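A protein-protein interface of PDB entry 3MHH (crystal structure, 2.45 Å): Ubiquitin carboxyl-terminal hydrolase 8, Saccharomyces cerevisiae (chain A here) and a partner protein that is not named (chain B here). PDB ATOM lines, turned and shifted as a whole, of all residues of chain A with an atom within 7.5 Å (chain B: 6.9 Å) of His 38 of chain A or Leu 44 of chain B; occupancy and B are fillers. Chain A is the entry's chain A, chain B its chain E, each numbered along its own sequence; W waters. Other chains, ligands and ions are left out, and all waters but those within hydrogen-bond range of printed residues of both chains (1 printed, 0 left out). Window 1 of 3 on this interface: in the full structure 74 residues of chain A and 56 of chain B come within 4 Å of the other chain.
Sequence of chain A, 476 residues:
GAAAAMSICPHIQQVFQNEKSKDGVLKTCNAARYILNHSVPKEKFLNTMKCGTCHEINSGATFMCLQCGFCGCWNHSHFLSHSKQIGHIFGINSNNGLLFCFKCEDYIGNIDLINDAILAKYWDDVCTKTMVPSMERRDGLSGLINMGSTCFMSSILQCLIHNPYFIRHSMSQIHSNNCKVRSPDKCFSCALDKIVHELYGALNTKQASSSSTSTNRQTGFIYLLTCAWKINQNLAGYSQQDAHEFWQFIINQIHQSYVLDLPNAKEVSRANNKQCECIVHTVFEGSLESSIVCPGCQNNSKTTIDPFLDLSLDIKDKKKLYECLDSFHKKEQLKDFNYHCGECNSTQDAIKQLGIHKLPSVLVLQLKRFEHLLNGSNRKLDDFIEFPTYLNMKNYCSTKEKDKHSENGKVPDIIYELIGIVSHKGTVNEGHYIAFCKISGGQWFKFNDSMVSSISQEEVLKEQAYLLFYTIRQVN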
ATOM      1  N   ALA A  32      29.121  23.905 -18.107  1.00  0.00           N
ATOM      2  CA  ALA A  32      28.492  23.010 -19.054  1.00  0.00           C
ATOM      3  C   ALA A  32      27.369  23.736 -19.777  1.00  0.00           C
ATOM      4  O   ALA A  32      27.216  23.614 -20.994  1.00  0.00           O
ATOM      5  CB  ALA A  32      27.957  21.787 -18.336  1.00  0.00           C
ATOM      6  N   ARG A  33      26.572  24.483 -19.028  1.00  0.00           N
ATOM      7  CA  ARG A  33      25.434  25.151 -19.624  1.00  0.00           C
ATOM      8  C   ARG A  33      25.927  26.220 -20.574  1.00  0.00           C
ATOM      9  O   ARG A  33      25.410  26.372 -21.678  1.00  0.00           O
ATOM     10  CB  ARG A  33      24.503  25.713 -18.551  1.00  0.00           C
ATOM     11  CG  ARG A  33      23.724  24.603 -17.837  1.00  0.00           C
ATOM     12  CD  ARG A  33      22.893  25.074 -16.629  1.00  0.00           C
ATOM     13  NE  ARG A  33      22.364  23.923 -15.889  1.00  0.00           N
ATOM     14  CZ  ARG A  33      21.770  23.987 -14.696  1.00  0.00           C
ATOM     15  NH1 ARG A  33      21.621  25.152 -14.085  1.00  0.00           N
ATOM     16  NH2 ARG A  33      21.319  22.883 -14.106  1.00  0.00           N
ATOM     17  N   TYR A  34      26.978  26.920 -20.175  1.00  0.00           N
ATOM     18  CA  TYR A  34      27.528  27.961 -21.014  1.00  0.00           C
ATOM     19  C   TYR A  34      27.954  27.352 -22.340  1.00  0.00           C
ATOM     20  O   TYR A  34      27.598  27.854 -23.403  1.00  0.00           O
ATOM     21  CB  TYR A  34      28.707  28.674 -20.332  1.00  0.00           C
ATOM     22  CG  TYR A  34      29.255  29.796 -21.173  1.00  0.00           C
ATOM     23  CD1 TYR A  34      28.693  31.078 -21.116  1.00  0.00           C
ATOM     24  CD2 TYR A  34      30.293  29.573 -22.068  1.00  0.00           C
ATOM     25  CE1 TYR A  34      29.176  32.108 -21.903  1.00  0.00           C
ATOM     26  CE2 TYR A  34      30.796  30.610 -22.854  1.00  0.00           C
ATOM     27  CZ  TYR A  34      30.227  31.867 -22.772  1.00  0.00           C
ATOM     28  OH  TYR A  34      30.707  32.876 -23.574  1.00  0.00           O
ATOM     29  N   ILE A  35      28.666  26.233 -22.279  1.00  0.00           N
ATOM     30  CA  ILE A  35      29.130  25.590 -23.494  1.00  0.00           C
ATOM     31  C   ILE A  35      27.956  25.185 -24.390  1.00  0.00           C
ATOM     32  O   ILE A  35      28.015  25.331 -25.607  1.00  0.00           O
ATOM     33  CB  ILE A  35      29.970  24.362 -23.174  1.00  0.00           C
ATOM     34  CG1 ILE A  35      31.331  24.787 -22.617  1.00  0.00           C
ATOM     35  CG2 ILE A  35      30.115  23.484 -24.411  1.00  0.00           C
ATOM     36  CD1 ILE A  35      32.099  23.654 -21.951  1.00  0.00           C
ATOM     37  N   LEU A  36      26.881  24.678 -23.800  1.00  0.00           N
ATOM     38  CA  LEU A  36      25.747  24.244 -24.616  1.00  0.00           C
ATOM     39  C   LEU A  36      25.127  25.416 -25.362  1.00  0.00           C
ATOM     40  O   LEU A  36      24.641  25.250 -26.455  1.00  0.00           O
ATOM     41  CB  LEU A  36      24.682  23.545 -23.770  1.00  0.00           C
ATOM     42  CG  LEU A  36      25.200  22.373 -22.942  1.00  0.00           C
ATOM     43  CD1 LEU A  36      24.154  21.958 -21.887  1.00  0.00           C
ATOM     44  CD2 LEU A  36      25.592  21.214 -23.844  1.00  0.00           C
ATOM     45  N   ASN A  37      25.166  26.603 -24.774  1.00  0.00           N
ATOM     46  CA  ASN A  37      24.627  27.816 -25.406  1.00  0.00           C
ATOM     47  C   ASN A  37      25.570  28.557 -26.381  1.00  0.00           C
ATOM     48  O   ASN A  37      25.168  29.545 -27.008  1.00  0.00           O
ATOM     49  CB  ASN A  37      24.207  28.797 -24.310  1.00  0.00           C
ATOM     50  CG  ASN A  37      22.796  28.554 -23.824  1.00  0.00           C
ATOM     51  OD1 ASN A  37      22.522  27.602 -23.084  1.00  0.00           O
ATOM     52  ND2 ASN A  37      21.883  29.429 -24.232  1.00  0.00           N
ATOM     53  N   HIS A  38      26.812  28.096 -26.502  1.00  0.00           N
ATOM     54  CA  HIS A  38      27.810  28.773 -27.322  1.00  0.00           C
ATOM     55  C   HIS A  38      28.606  27.781 -28.156  1.00  0.00           C
ATOM     56  O   HIS A  38      29.800  27.973 -28.399  1.00  0.00           O
ATOM     57  CB  HIS A  38      28.758  29.596 -26.438  1.00  0.00           C
ATOM     58  CG  HIS A  38      28.058  30.649 -25.638  1.00  0.00           C
ATOM     59  ND1 HIS A  38      28.071  31.976 -25.992  1.00  0.00           N
ATOM     60  CD2 HIS A  38      27.264  30.560 -24.548  1.00  0.00           C
ATOM     61  CE1 HIS A  38      27.342  32.667 -25.137  1.00  0.00           C
ATOM     62  NE2 HIS A  38      26.828  31.830 -24.257  1.00  0.00           N
ATOM     63  N   SER A  39      27.930  26.710 -28.552  1.00  0.00           N
ATOM     64  CA  SER A  39      28.465  25.694 -29.449  1.00  0.00           C
ATOM     65  C   SER A  39      27.616  25.666 -30.714  1.00  0.00           C
ATOM     66  O   SER A  39      26.388  25.559 -30.638  1.00  0.00           O
ATOM     67  CB  SER A  39      28.361  24.314 -28.803  1.00  0.00           C
ATOM     68  OG  SER A  39      29.246  24.156 -27.721  1.00  0.00           O
ATOM     69  N   VAL A  40      28.268  25.761 -31.870  1.00  0.00           N
ATOM     70  CA  VAL A  40      27.585  25.628 -33.133  1.00  0.00           C
ATOM     71  C   VAL A  40      27.120  24.184 -33.245  1.00  0.00           C
ATOM     72  O   VAL A  40      27.687  23.303 -32.595  1.00  0.00           O
ATOM     73  CB  VAL A  40      28.492  25.992 -34.313  1.00  0.00           C
ATOM     74  CG1 VAL A  40      28.913  27.480 -34.246  1.00  0.00           C
ATOM     75  CG2 VAL A  40      29.695  25.080 -34.372  1.00  0.00           C
ATOM     76  N   PRO A  41      26.060  23.943 -34.036  1.00  0.00           N
ATOM     77  CA  PRO A  41      25.404  22.637 -34.133  1.00  0.00           C
ATOM     78  C   PRO A  41      26.317  21.434 -34.256  1.00  0.00           C
ATOM     79  O   PRO A  41      26.140  20.459 -33.513  1.00  0.00           O
ATOM     80  CB  PRO A  41      24.518  22.791 -35.371  1.00  0.00           C
ATOM     81  CG  PRO A  41      24.100  24.245 -35.307  1.00  0.00           C
ATOM     82  CD  PRO A  41      25.350  24.970 -34.827  1.00  0.00           C
ATOM     83  N   GLU A  43      29.586  21.111 -33.581  1.00  0.00           N
ATOM     84  CA  GLU A  43      30.395  20.976 -32.378  1.00  0.00           C
ATOM     85  C   GLU A  43      29.571  20.352 -31.268  1.00  0.00           C
ATOM     86  O   GLU A  43      30.028  19.462 -30.552  1.00  0.00           O
ATOM     87  CB  GLU A  43      30.823  22.347 -31.889  1.00  0.00           C
ATOM     88  CG  GLU A  43      31.978  22.973 -32.625  1.00  0.00           C
ATOM     89  CD  GLU A  43      32.394  24.256 -31.963  1.00  0.00           C
ATOM     90  OE1 GLU A  43      33.613  24.494 -31.871  1.00  0.00           O
ATOM     91  OE2 GLU A  43      31.494  25.000 -31.491  1.00  0.00           O
ATOM     92  N   LYS A  44      28.346  20.852 -31.117  1.00  0.00           N
ATOM     93  CA  LYS A  44      27.471  20.403 -30.046  1.00  0.00           C
ATOM     94  C   LYS A  44      27.181  18.916 -30.199  1.00  0.00           C
ATOM     95  O   LYS A  44      27.267  18.169 -29.229  1.00  0.00           O
ATOM     96  CB  LYS A  44      26.182  21.207 -30.064  1.00  0.00           C
ATOM     97  CG  LYS A  44      25.429  21.266 -28.772  1.00  0.00           C
ATOM     98  CD  LYS A  44      24.195  22.164 -28.940  1.00  0.00           C
ATOM     99  CE  LYS A  44      23.315  22.223 -27.699  1.00  0.00           C
ATOM    100  NZ  LYS A  44      21.943  22.742 -28.044  1.00  0.00           N
ATOM    101  N   LEU B  35      36.108  22.325 -24.389  1.00  0.00           N
ATOM    102  CA  LEU B  35      35.339  23.135 -25.319  1.00  0.00           C
ATOM    103  C   LEU B  35      35.244  24.587 -24.903  1.00  0.00           C
ATOM    104  O   LEU B  35      34.741  25.419 -25.658  1.00  0.00           O
ATOM    105  CB  LEU B  35      33.921  22.577 -25.418  1.00  0.00           C
ATOM    106  CG  LEU B  35      33.761  21.295 -26.227  1.00  0.00           C
ATOM    107  CD1 LEU B  35      32.396  20.636 -25.924  1.00  0.00           C
ATOM    108  CD2 LEU B  35      33.906  21.623 -27.713  1.00  0.00           C
ATOM    109  N   SER B  38      36.623  27.528 -27.159  1.00  0.00           N
ATOM    110  CA  SER B  38      35.861  27.738 -28.372  1.00  0.00           C
ATOM    111  C   SER B  38      34.496  28.356 -28.025  1.00  0.00           C
ATOM    112  O   SER B  38      34.034  29.295 -28.683  1.00  0.00           O
ATOM    113  CB  SER B  38      35.701  26.407 -29.116  1.00  0.00           C
ATOM    114  OG  SER B  38      34.751  26.516 -30.163  1.00  0.00           O
ATOM    115  N   ALA B  39      33.869  27.848 -26.974  1.00  0.00           N
ATOM    116  CA  ALA B  39      32.604  28.399 -26.491  1.00  0.00           C
ATOM    117  C   ALA B  39      32.682  29.892 -26.186  1.00  0.00           C
ATOM    118  O   ALA B  39      31.801  30.653 -26.565  1.00  0.00           O
ATOM    119  CB  ALA B  39      32.144  27.644 -25.245  1.00  0.00           C
ATOM    120  N   LYS B  40      33.726  30.313 -25.480  1.00  0.00           N
ATOM    121  CA  LYS B  40      33.872  31.730 -25.131  1.00  0.00           C
ATOM    122  C   LYS B  40      33.982  32.595 -26.390  1.00  0.00           C
ATOM    123  O   LYS B  40      33.481  33.712 -26.413  1.00  0.00           O
ATOM    124  CB  LYS B  40      35.088  31.952 -24.232  1.00  0.00           C
ATOM    125  CG  LYS B  40      34.869  31.607 -22.763  1.00  0.00           C
ATOM    126  CD  LYS B  40      36.167  31.708 -21.992  1.00  0.00           C
ATOM    127  CE  LYS B  40      35.954  31.834 -20.487  1.00  0.00           C
ATOM    128  NZ  LYS B  40      37.220  31.599 -19.704  1.00  0.00           N
ATOM    129  N   ASP B  41      34.638  32.071 -27.425  1.00  0.00           N
ATOM    130  CA  ASP B  41      34.811  32.775 -28.700  1.00  0.00           C
ATOM    131  C   ASP B  41      33.485  32.973 -29.427  1.00  0.00           C
ATOM    132  O   ASP B  41      33.348  33.887 -30.236  1.00  0.00           O
ATOM    133  CB  ASP B  41      35.694  31.954 -29.661  1.00  0.00           C
ATOM    134  CG  ASP B  41      37.150  31.939 -29.277  1.00  0.00           C
ATOM    135  OD1 ASP B  41      37.515  32.499 -28.224  1.00  0.00           O
ATOM    136  OD2 ASP B  41      37.942  31.335 -30.040  1.00  0.00           O
ATOM    137  N   THR B  42      32.533  32.089 -29.163  1.00  0.00           N
ATOM    138  CA  THR B  42      31.377  31.902 -30.033  1.00  0.00           C
ATOM    139  C   THR B  42      30.126  32.591 -29.516  1.00  0.00           C
ATOM    140  O   THR B  42      29.750  32.419 -28.355  1.00  0.00           O
ATOM    141  CB  THR B  42      31.058  30.403 -30.175  1.00  0.00           C
ATOM    142  OG1 THR B  42      32.165  29.725 -30.789  1.00  0.00           O
ATOM    143  CG2 THR B  42      29.811  30.186 -30.999  1.00  0.00           C
ATOM    144  N   PRO B  43      29.440  33.334 -30.395  1.00  0.00           N
ATOM    145  CA  PRO B  43      28.241  34.047 -29.998  1.00  0.00           C
ATOM    146  C   PRO B  43      27.121  33.112 -29.605  1.00  0.00           C
ATOM    147  O   PRO B  43      27.122  31.935 -29.979  1.00  0.00           O
ATOM    148  CB  PRO B  43      27.857  34.837 -31.243  1.00  0.00           C
ATOM    149  CG  PRO B  43      29.097  34.887 -32.073  1.00  0.00           C
ATOM    150  CD  PRO B  43      29.796  33.596 -31.796  1.00  0.00           C
ATOM    151  N   LEU B  44      26.164  33.655 -28.861  1.00  0.00           N
ATOM    152  CA  LEU B  44      25.058  32.888 -28.356  1.00  0.00           C
ATOM    153  C   LEU B  44      24.399  32.097 -29.487  1.00  0.00           C
ATOM    154  O   LEU B  44      24.047  32.673 -30.510  1.00  0.00           O
ATOM    155  CB  LEU B  44      24.061  33.847 -27.726  1.00  0.00           C
ATOM    156  CG  LEU B  44      22.889  33.235 -26.973  1.00  0.00           C
ATOM    157  CD1 LEU B  44      23.402  32.478 -25.747  1.00  0.00           C
ATOM    158  CD2 LEU B  44      21.920  34.365 -26.586  1.00  0.00           C
ATOM    159  N   GLN B  45      24.247  30.783 -29.301  1.00  0.00           N
ATOM    160  CA  GLN B  45      23.605  29.901 -30.294  1.00  0.00           C
ATOM    161  C   GLN B  45      22.259  29.380 -29.804  1.00  0.00           C
ATOM    162  O   GLN B  45      22.060  29.188 -28.618  1.00  0.00           O
ATOM    163  CB  GLN B  45      24.477  28.687 -30.613  1.00  0.00           C
ATOM    164  CG  GLN B  45      25.915  28.980 -30.979  1.00  0.00           C
ATOM    165  CD  GLN B  45      26.082  29.534 -32.384  1.00  0.00           C
ATOM    166  OE1 GLN B  45      25.561  28.972 -33.342  1.00  0.00           O
ATOM    167  NE2 GLN B  45      26.861  30.620 -32.514  1.00  0.00           N
ATOM    168  N   TYR B  46      21.353  29.114 -30.741  1.00  0.00           N
ATOM    169  CA  TYR B  46      20.051  28.542 -30.425  1.00  0.00           C
ATOM    170  C   TYR B  46      20.000  27.102 -30.883  1.00  0.00           C
ATOM    171  O   TYR B  46      20.609  26.727 -31.882  1.00  0.00           O
ATOM    172  CB  TYR B  46      18.928  29.369 -31.047  1.00  0.00           C
ATOM    173  CG  TYR B  46      19.000  30.801 -30.577  1.00  0.00           C
ATOM    174  CD1 TYR B  46      18.677  31.131 -29.273  1.00  0.00           C
ATOM    175  CD2 TYR B  46      19.469  31.809 -31.406  1.00  0.00           C
ATOM    176  CE1 TYR B  46      18.793  32.419 -28.818  1.00  0.00           C
ATOM    177  CE2 TYR B  46      19.594  33.104 -30.949  1.00  0.00           C
ATOM    178  CZ  TYR B  46      19.253  33.400 -29.654  1.00  0.00           C
ATOM    179  OH  TYR B  46      19.340  34.694 -29.185  1.00  0.00           O
ATOM    180  N   ARG B  51      21.253  30.257 -37.207  1.00  0.00           N
ATOM    181  CA  ARG B  51      21.899  31.556 -37.157  1.00  0.00           C
ATOM    182  C   ARG B  51      21.830  32.254 -38.499  1.00  0.00           C
ATOM    183  O   ARG B  51      21.499  33.437 -38.562  1.00  0.00           O
ATOM    184  CB  ARG B  51      23.345  31.424 -36.706  1.00  0.00           C
ATOM    185  CG  ARG B  51      24.064  32.750 -36.577  1.00  0.00           C
ATOM    186  CD  ARG B  51      25.491  32.543 -36.106  1.00  0.00           C
ATOM    187  NE  ARG B  51      26.225  33.799 -36.032  1.00  0.00           N
ATOM    188  CZ  ARG B  51      26.081  34.686 -35.053  1.00  0.00           C
ATOM    189  NH1 ARG B  51      25.214  34.460 -34.068  1.00  0.00           N
ATOM    190  NH2 ARG B  51      26.789  35.811 -35.070  1.00  0.00           N
ATOM    191  N   LEU B  64      15.448  37.510 -28.923  1.00  0.00           N
ATOM    192  CA  LEU B  64      15.097  36.135 -29.181  1.00  0.00           C
ATOM    193  C   LEU B  64      15.091  35.330 -27.896  1.00  0.00           C
ATOM    194  O   LEU B  64      16.093  35.259 -27.198  1.00  0.00           O
ATOM    195  CB  LEU B  64      16.074  35.528 -30.195  1.00  0.00           C
ATOM    196  CG  LEU B  64      15.960  36.058 -31.625  1.00  0.00           C
ATOM    197  CD1 LEU B  64      17.105  35.544 -32.478  1.00  0.00           C
ATOM    198  CD2 LEU B  64      14.612  35.662 -32.245  1.00  0.00           C
HETATM  199  O   HOH W   1      23.583  25.275 -31.529  1.00  0.00           O
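Water W1 lies within hydrogen-bond range of the backbone carbonyl oxygen of Ser 39 of chain A (3.0 Å) and the backbone carbonyl oxygen of Tyr 46 of chain B (3.3 Å).
Of the 12 printed residues of chain B, 8 touch a printed residue of chain A.
Hydrophobic or aromatic side chains of chain B that line the printed part of chain A: Leu 35, Ala 39 and Leu 44.
Hydrophobic or aromatic side chains of chain A that line the printed part of chain B: Tyr 34, Ile 35, His 38 and Val 40.
Among the printed residues, no Asp or Glu carboxylate lies within 4 Å of a Lys or Arg side-chain nitrogen of the other chain.
OG of Ser 38 of chain B sits at hydrogen-bond distance from OE1 of Glu 43 of chain A (2.9 Å).
ND1 of His 38 of chain A lies within hydrogen-bond range of O of Thr 42 of chain B, 2.9 Å away.
N of Gln 45 of chain B is in hydrogen-bond range of O of Asn 37 of chain A.
Of chain B, only Ala 39 (3.2 Å), Thr 42 (2.9 Å), Pro 43 (3.9 Å) and Leu 44 (3.8 Å) come within 4 Å of His 38 of chain A.
Of chain A, only Asn 37 and His 38 come within 4 Å of Leu 44 of chain B.
Of the printed residues of chain A, Leu 35 of chain B touches Ile 35.
Printed residues of chain B within 4 Å of Val 40 of chain A: Gln 45 (3.8 Å).
Of the printed residues of chain B, Ser 39 of chain A touches Gln 45 (3.5 Å).
Printed residues of chain A within 4 Å of Ser 38 of chain B: Glu 43 (2.9 Å).
Printed residues of chain A within 4 Å of Pro 43 of chain B: His 38 (3.9 Å).
The nearest residue of chain B that does not touch His 38 of chain A is Gln 45 of chain B (4.1 Å).
CE2 of Tyr 34 of chain A touches O of Ala 39 of chain B, at 3.8 Å.
OH of Tyr 34 of chain A touches CA of Lys 40 of chain B, at 3.7 Å.
Ile 35 of chain A touches Leu 35 of chain B.
Ile 35 of chain A touches Ala 39 of chain B (CG1 to CB, 3.97 Å).
Asn 37 of chain A touches Leu 44 of chain B (O to CA, 3.6 Å).
Ala 39 of chain B touches His 38 of chain A (O to CB, 3.2 Å).
His 38 of chain A touches Pro 43 of chain B (ND1 to C, 3.9 Å).
His 38 of chain A touches Leu 44 of chain B (NE2 to CD1, 3.8 Å).
Ser 39 of chain A touches Gln 45 of chain B.
CG1 of Val 40 of chain A touches OE1 of Gln 45 of chain B (3.8 Å).
OE2 of Glu 43 of chain A sits at hydrogen-bond distance from N of Val 40 of chain A, 3.3 Å away.
OG of Ser 39 of chain A lies within hydrogen-bond range of O of Ile 35 of chain A, 2.7 Å away.
O of Arg 33 of chain A sits close to OD1 of Asn 37 of chain A, at 3.4 Å.
O of Ser 38 of chain B is in hydrogen-bond range of OG1 of Thr 42 of chain B, at 2.8 Å.
O of Pro 43 of chain B is in hydrogen-bond range of NE2 of Gln 45 of chain B, at 2.9 Å.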
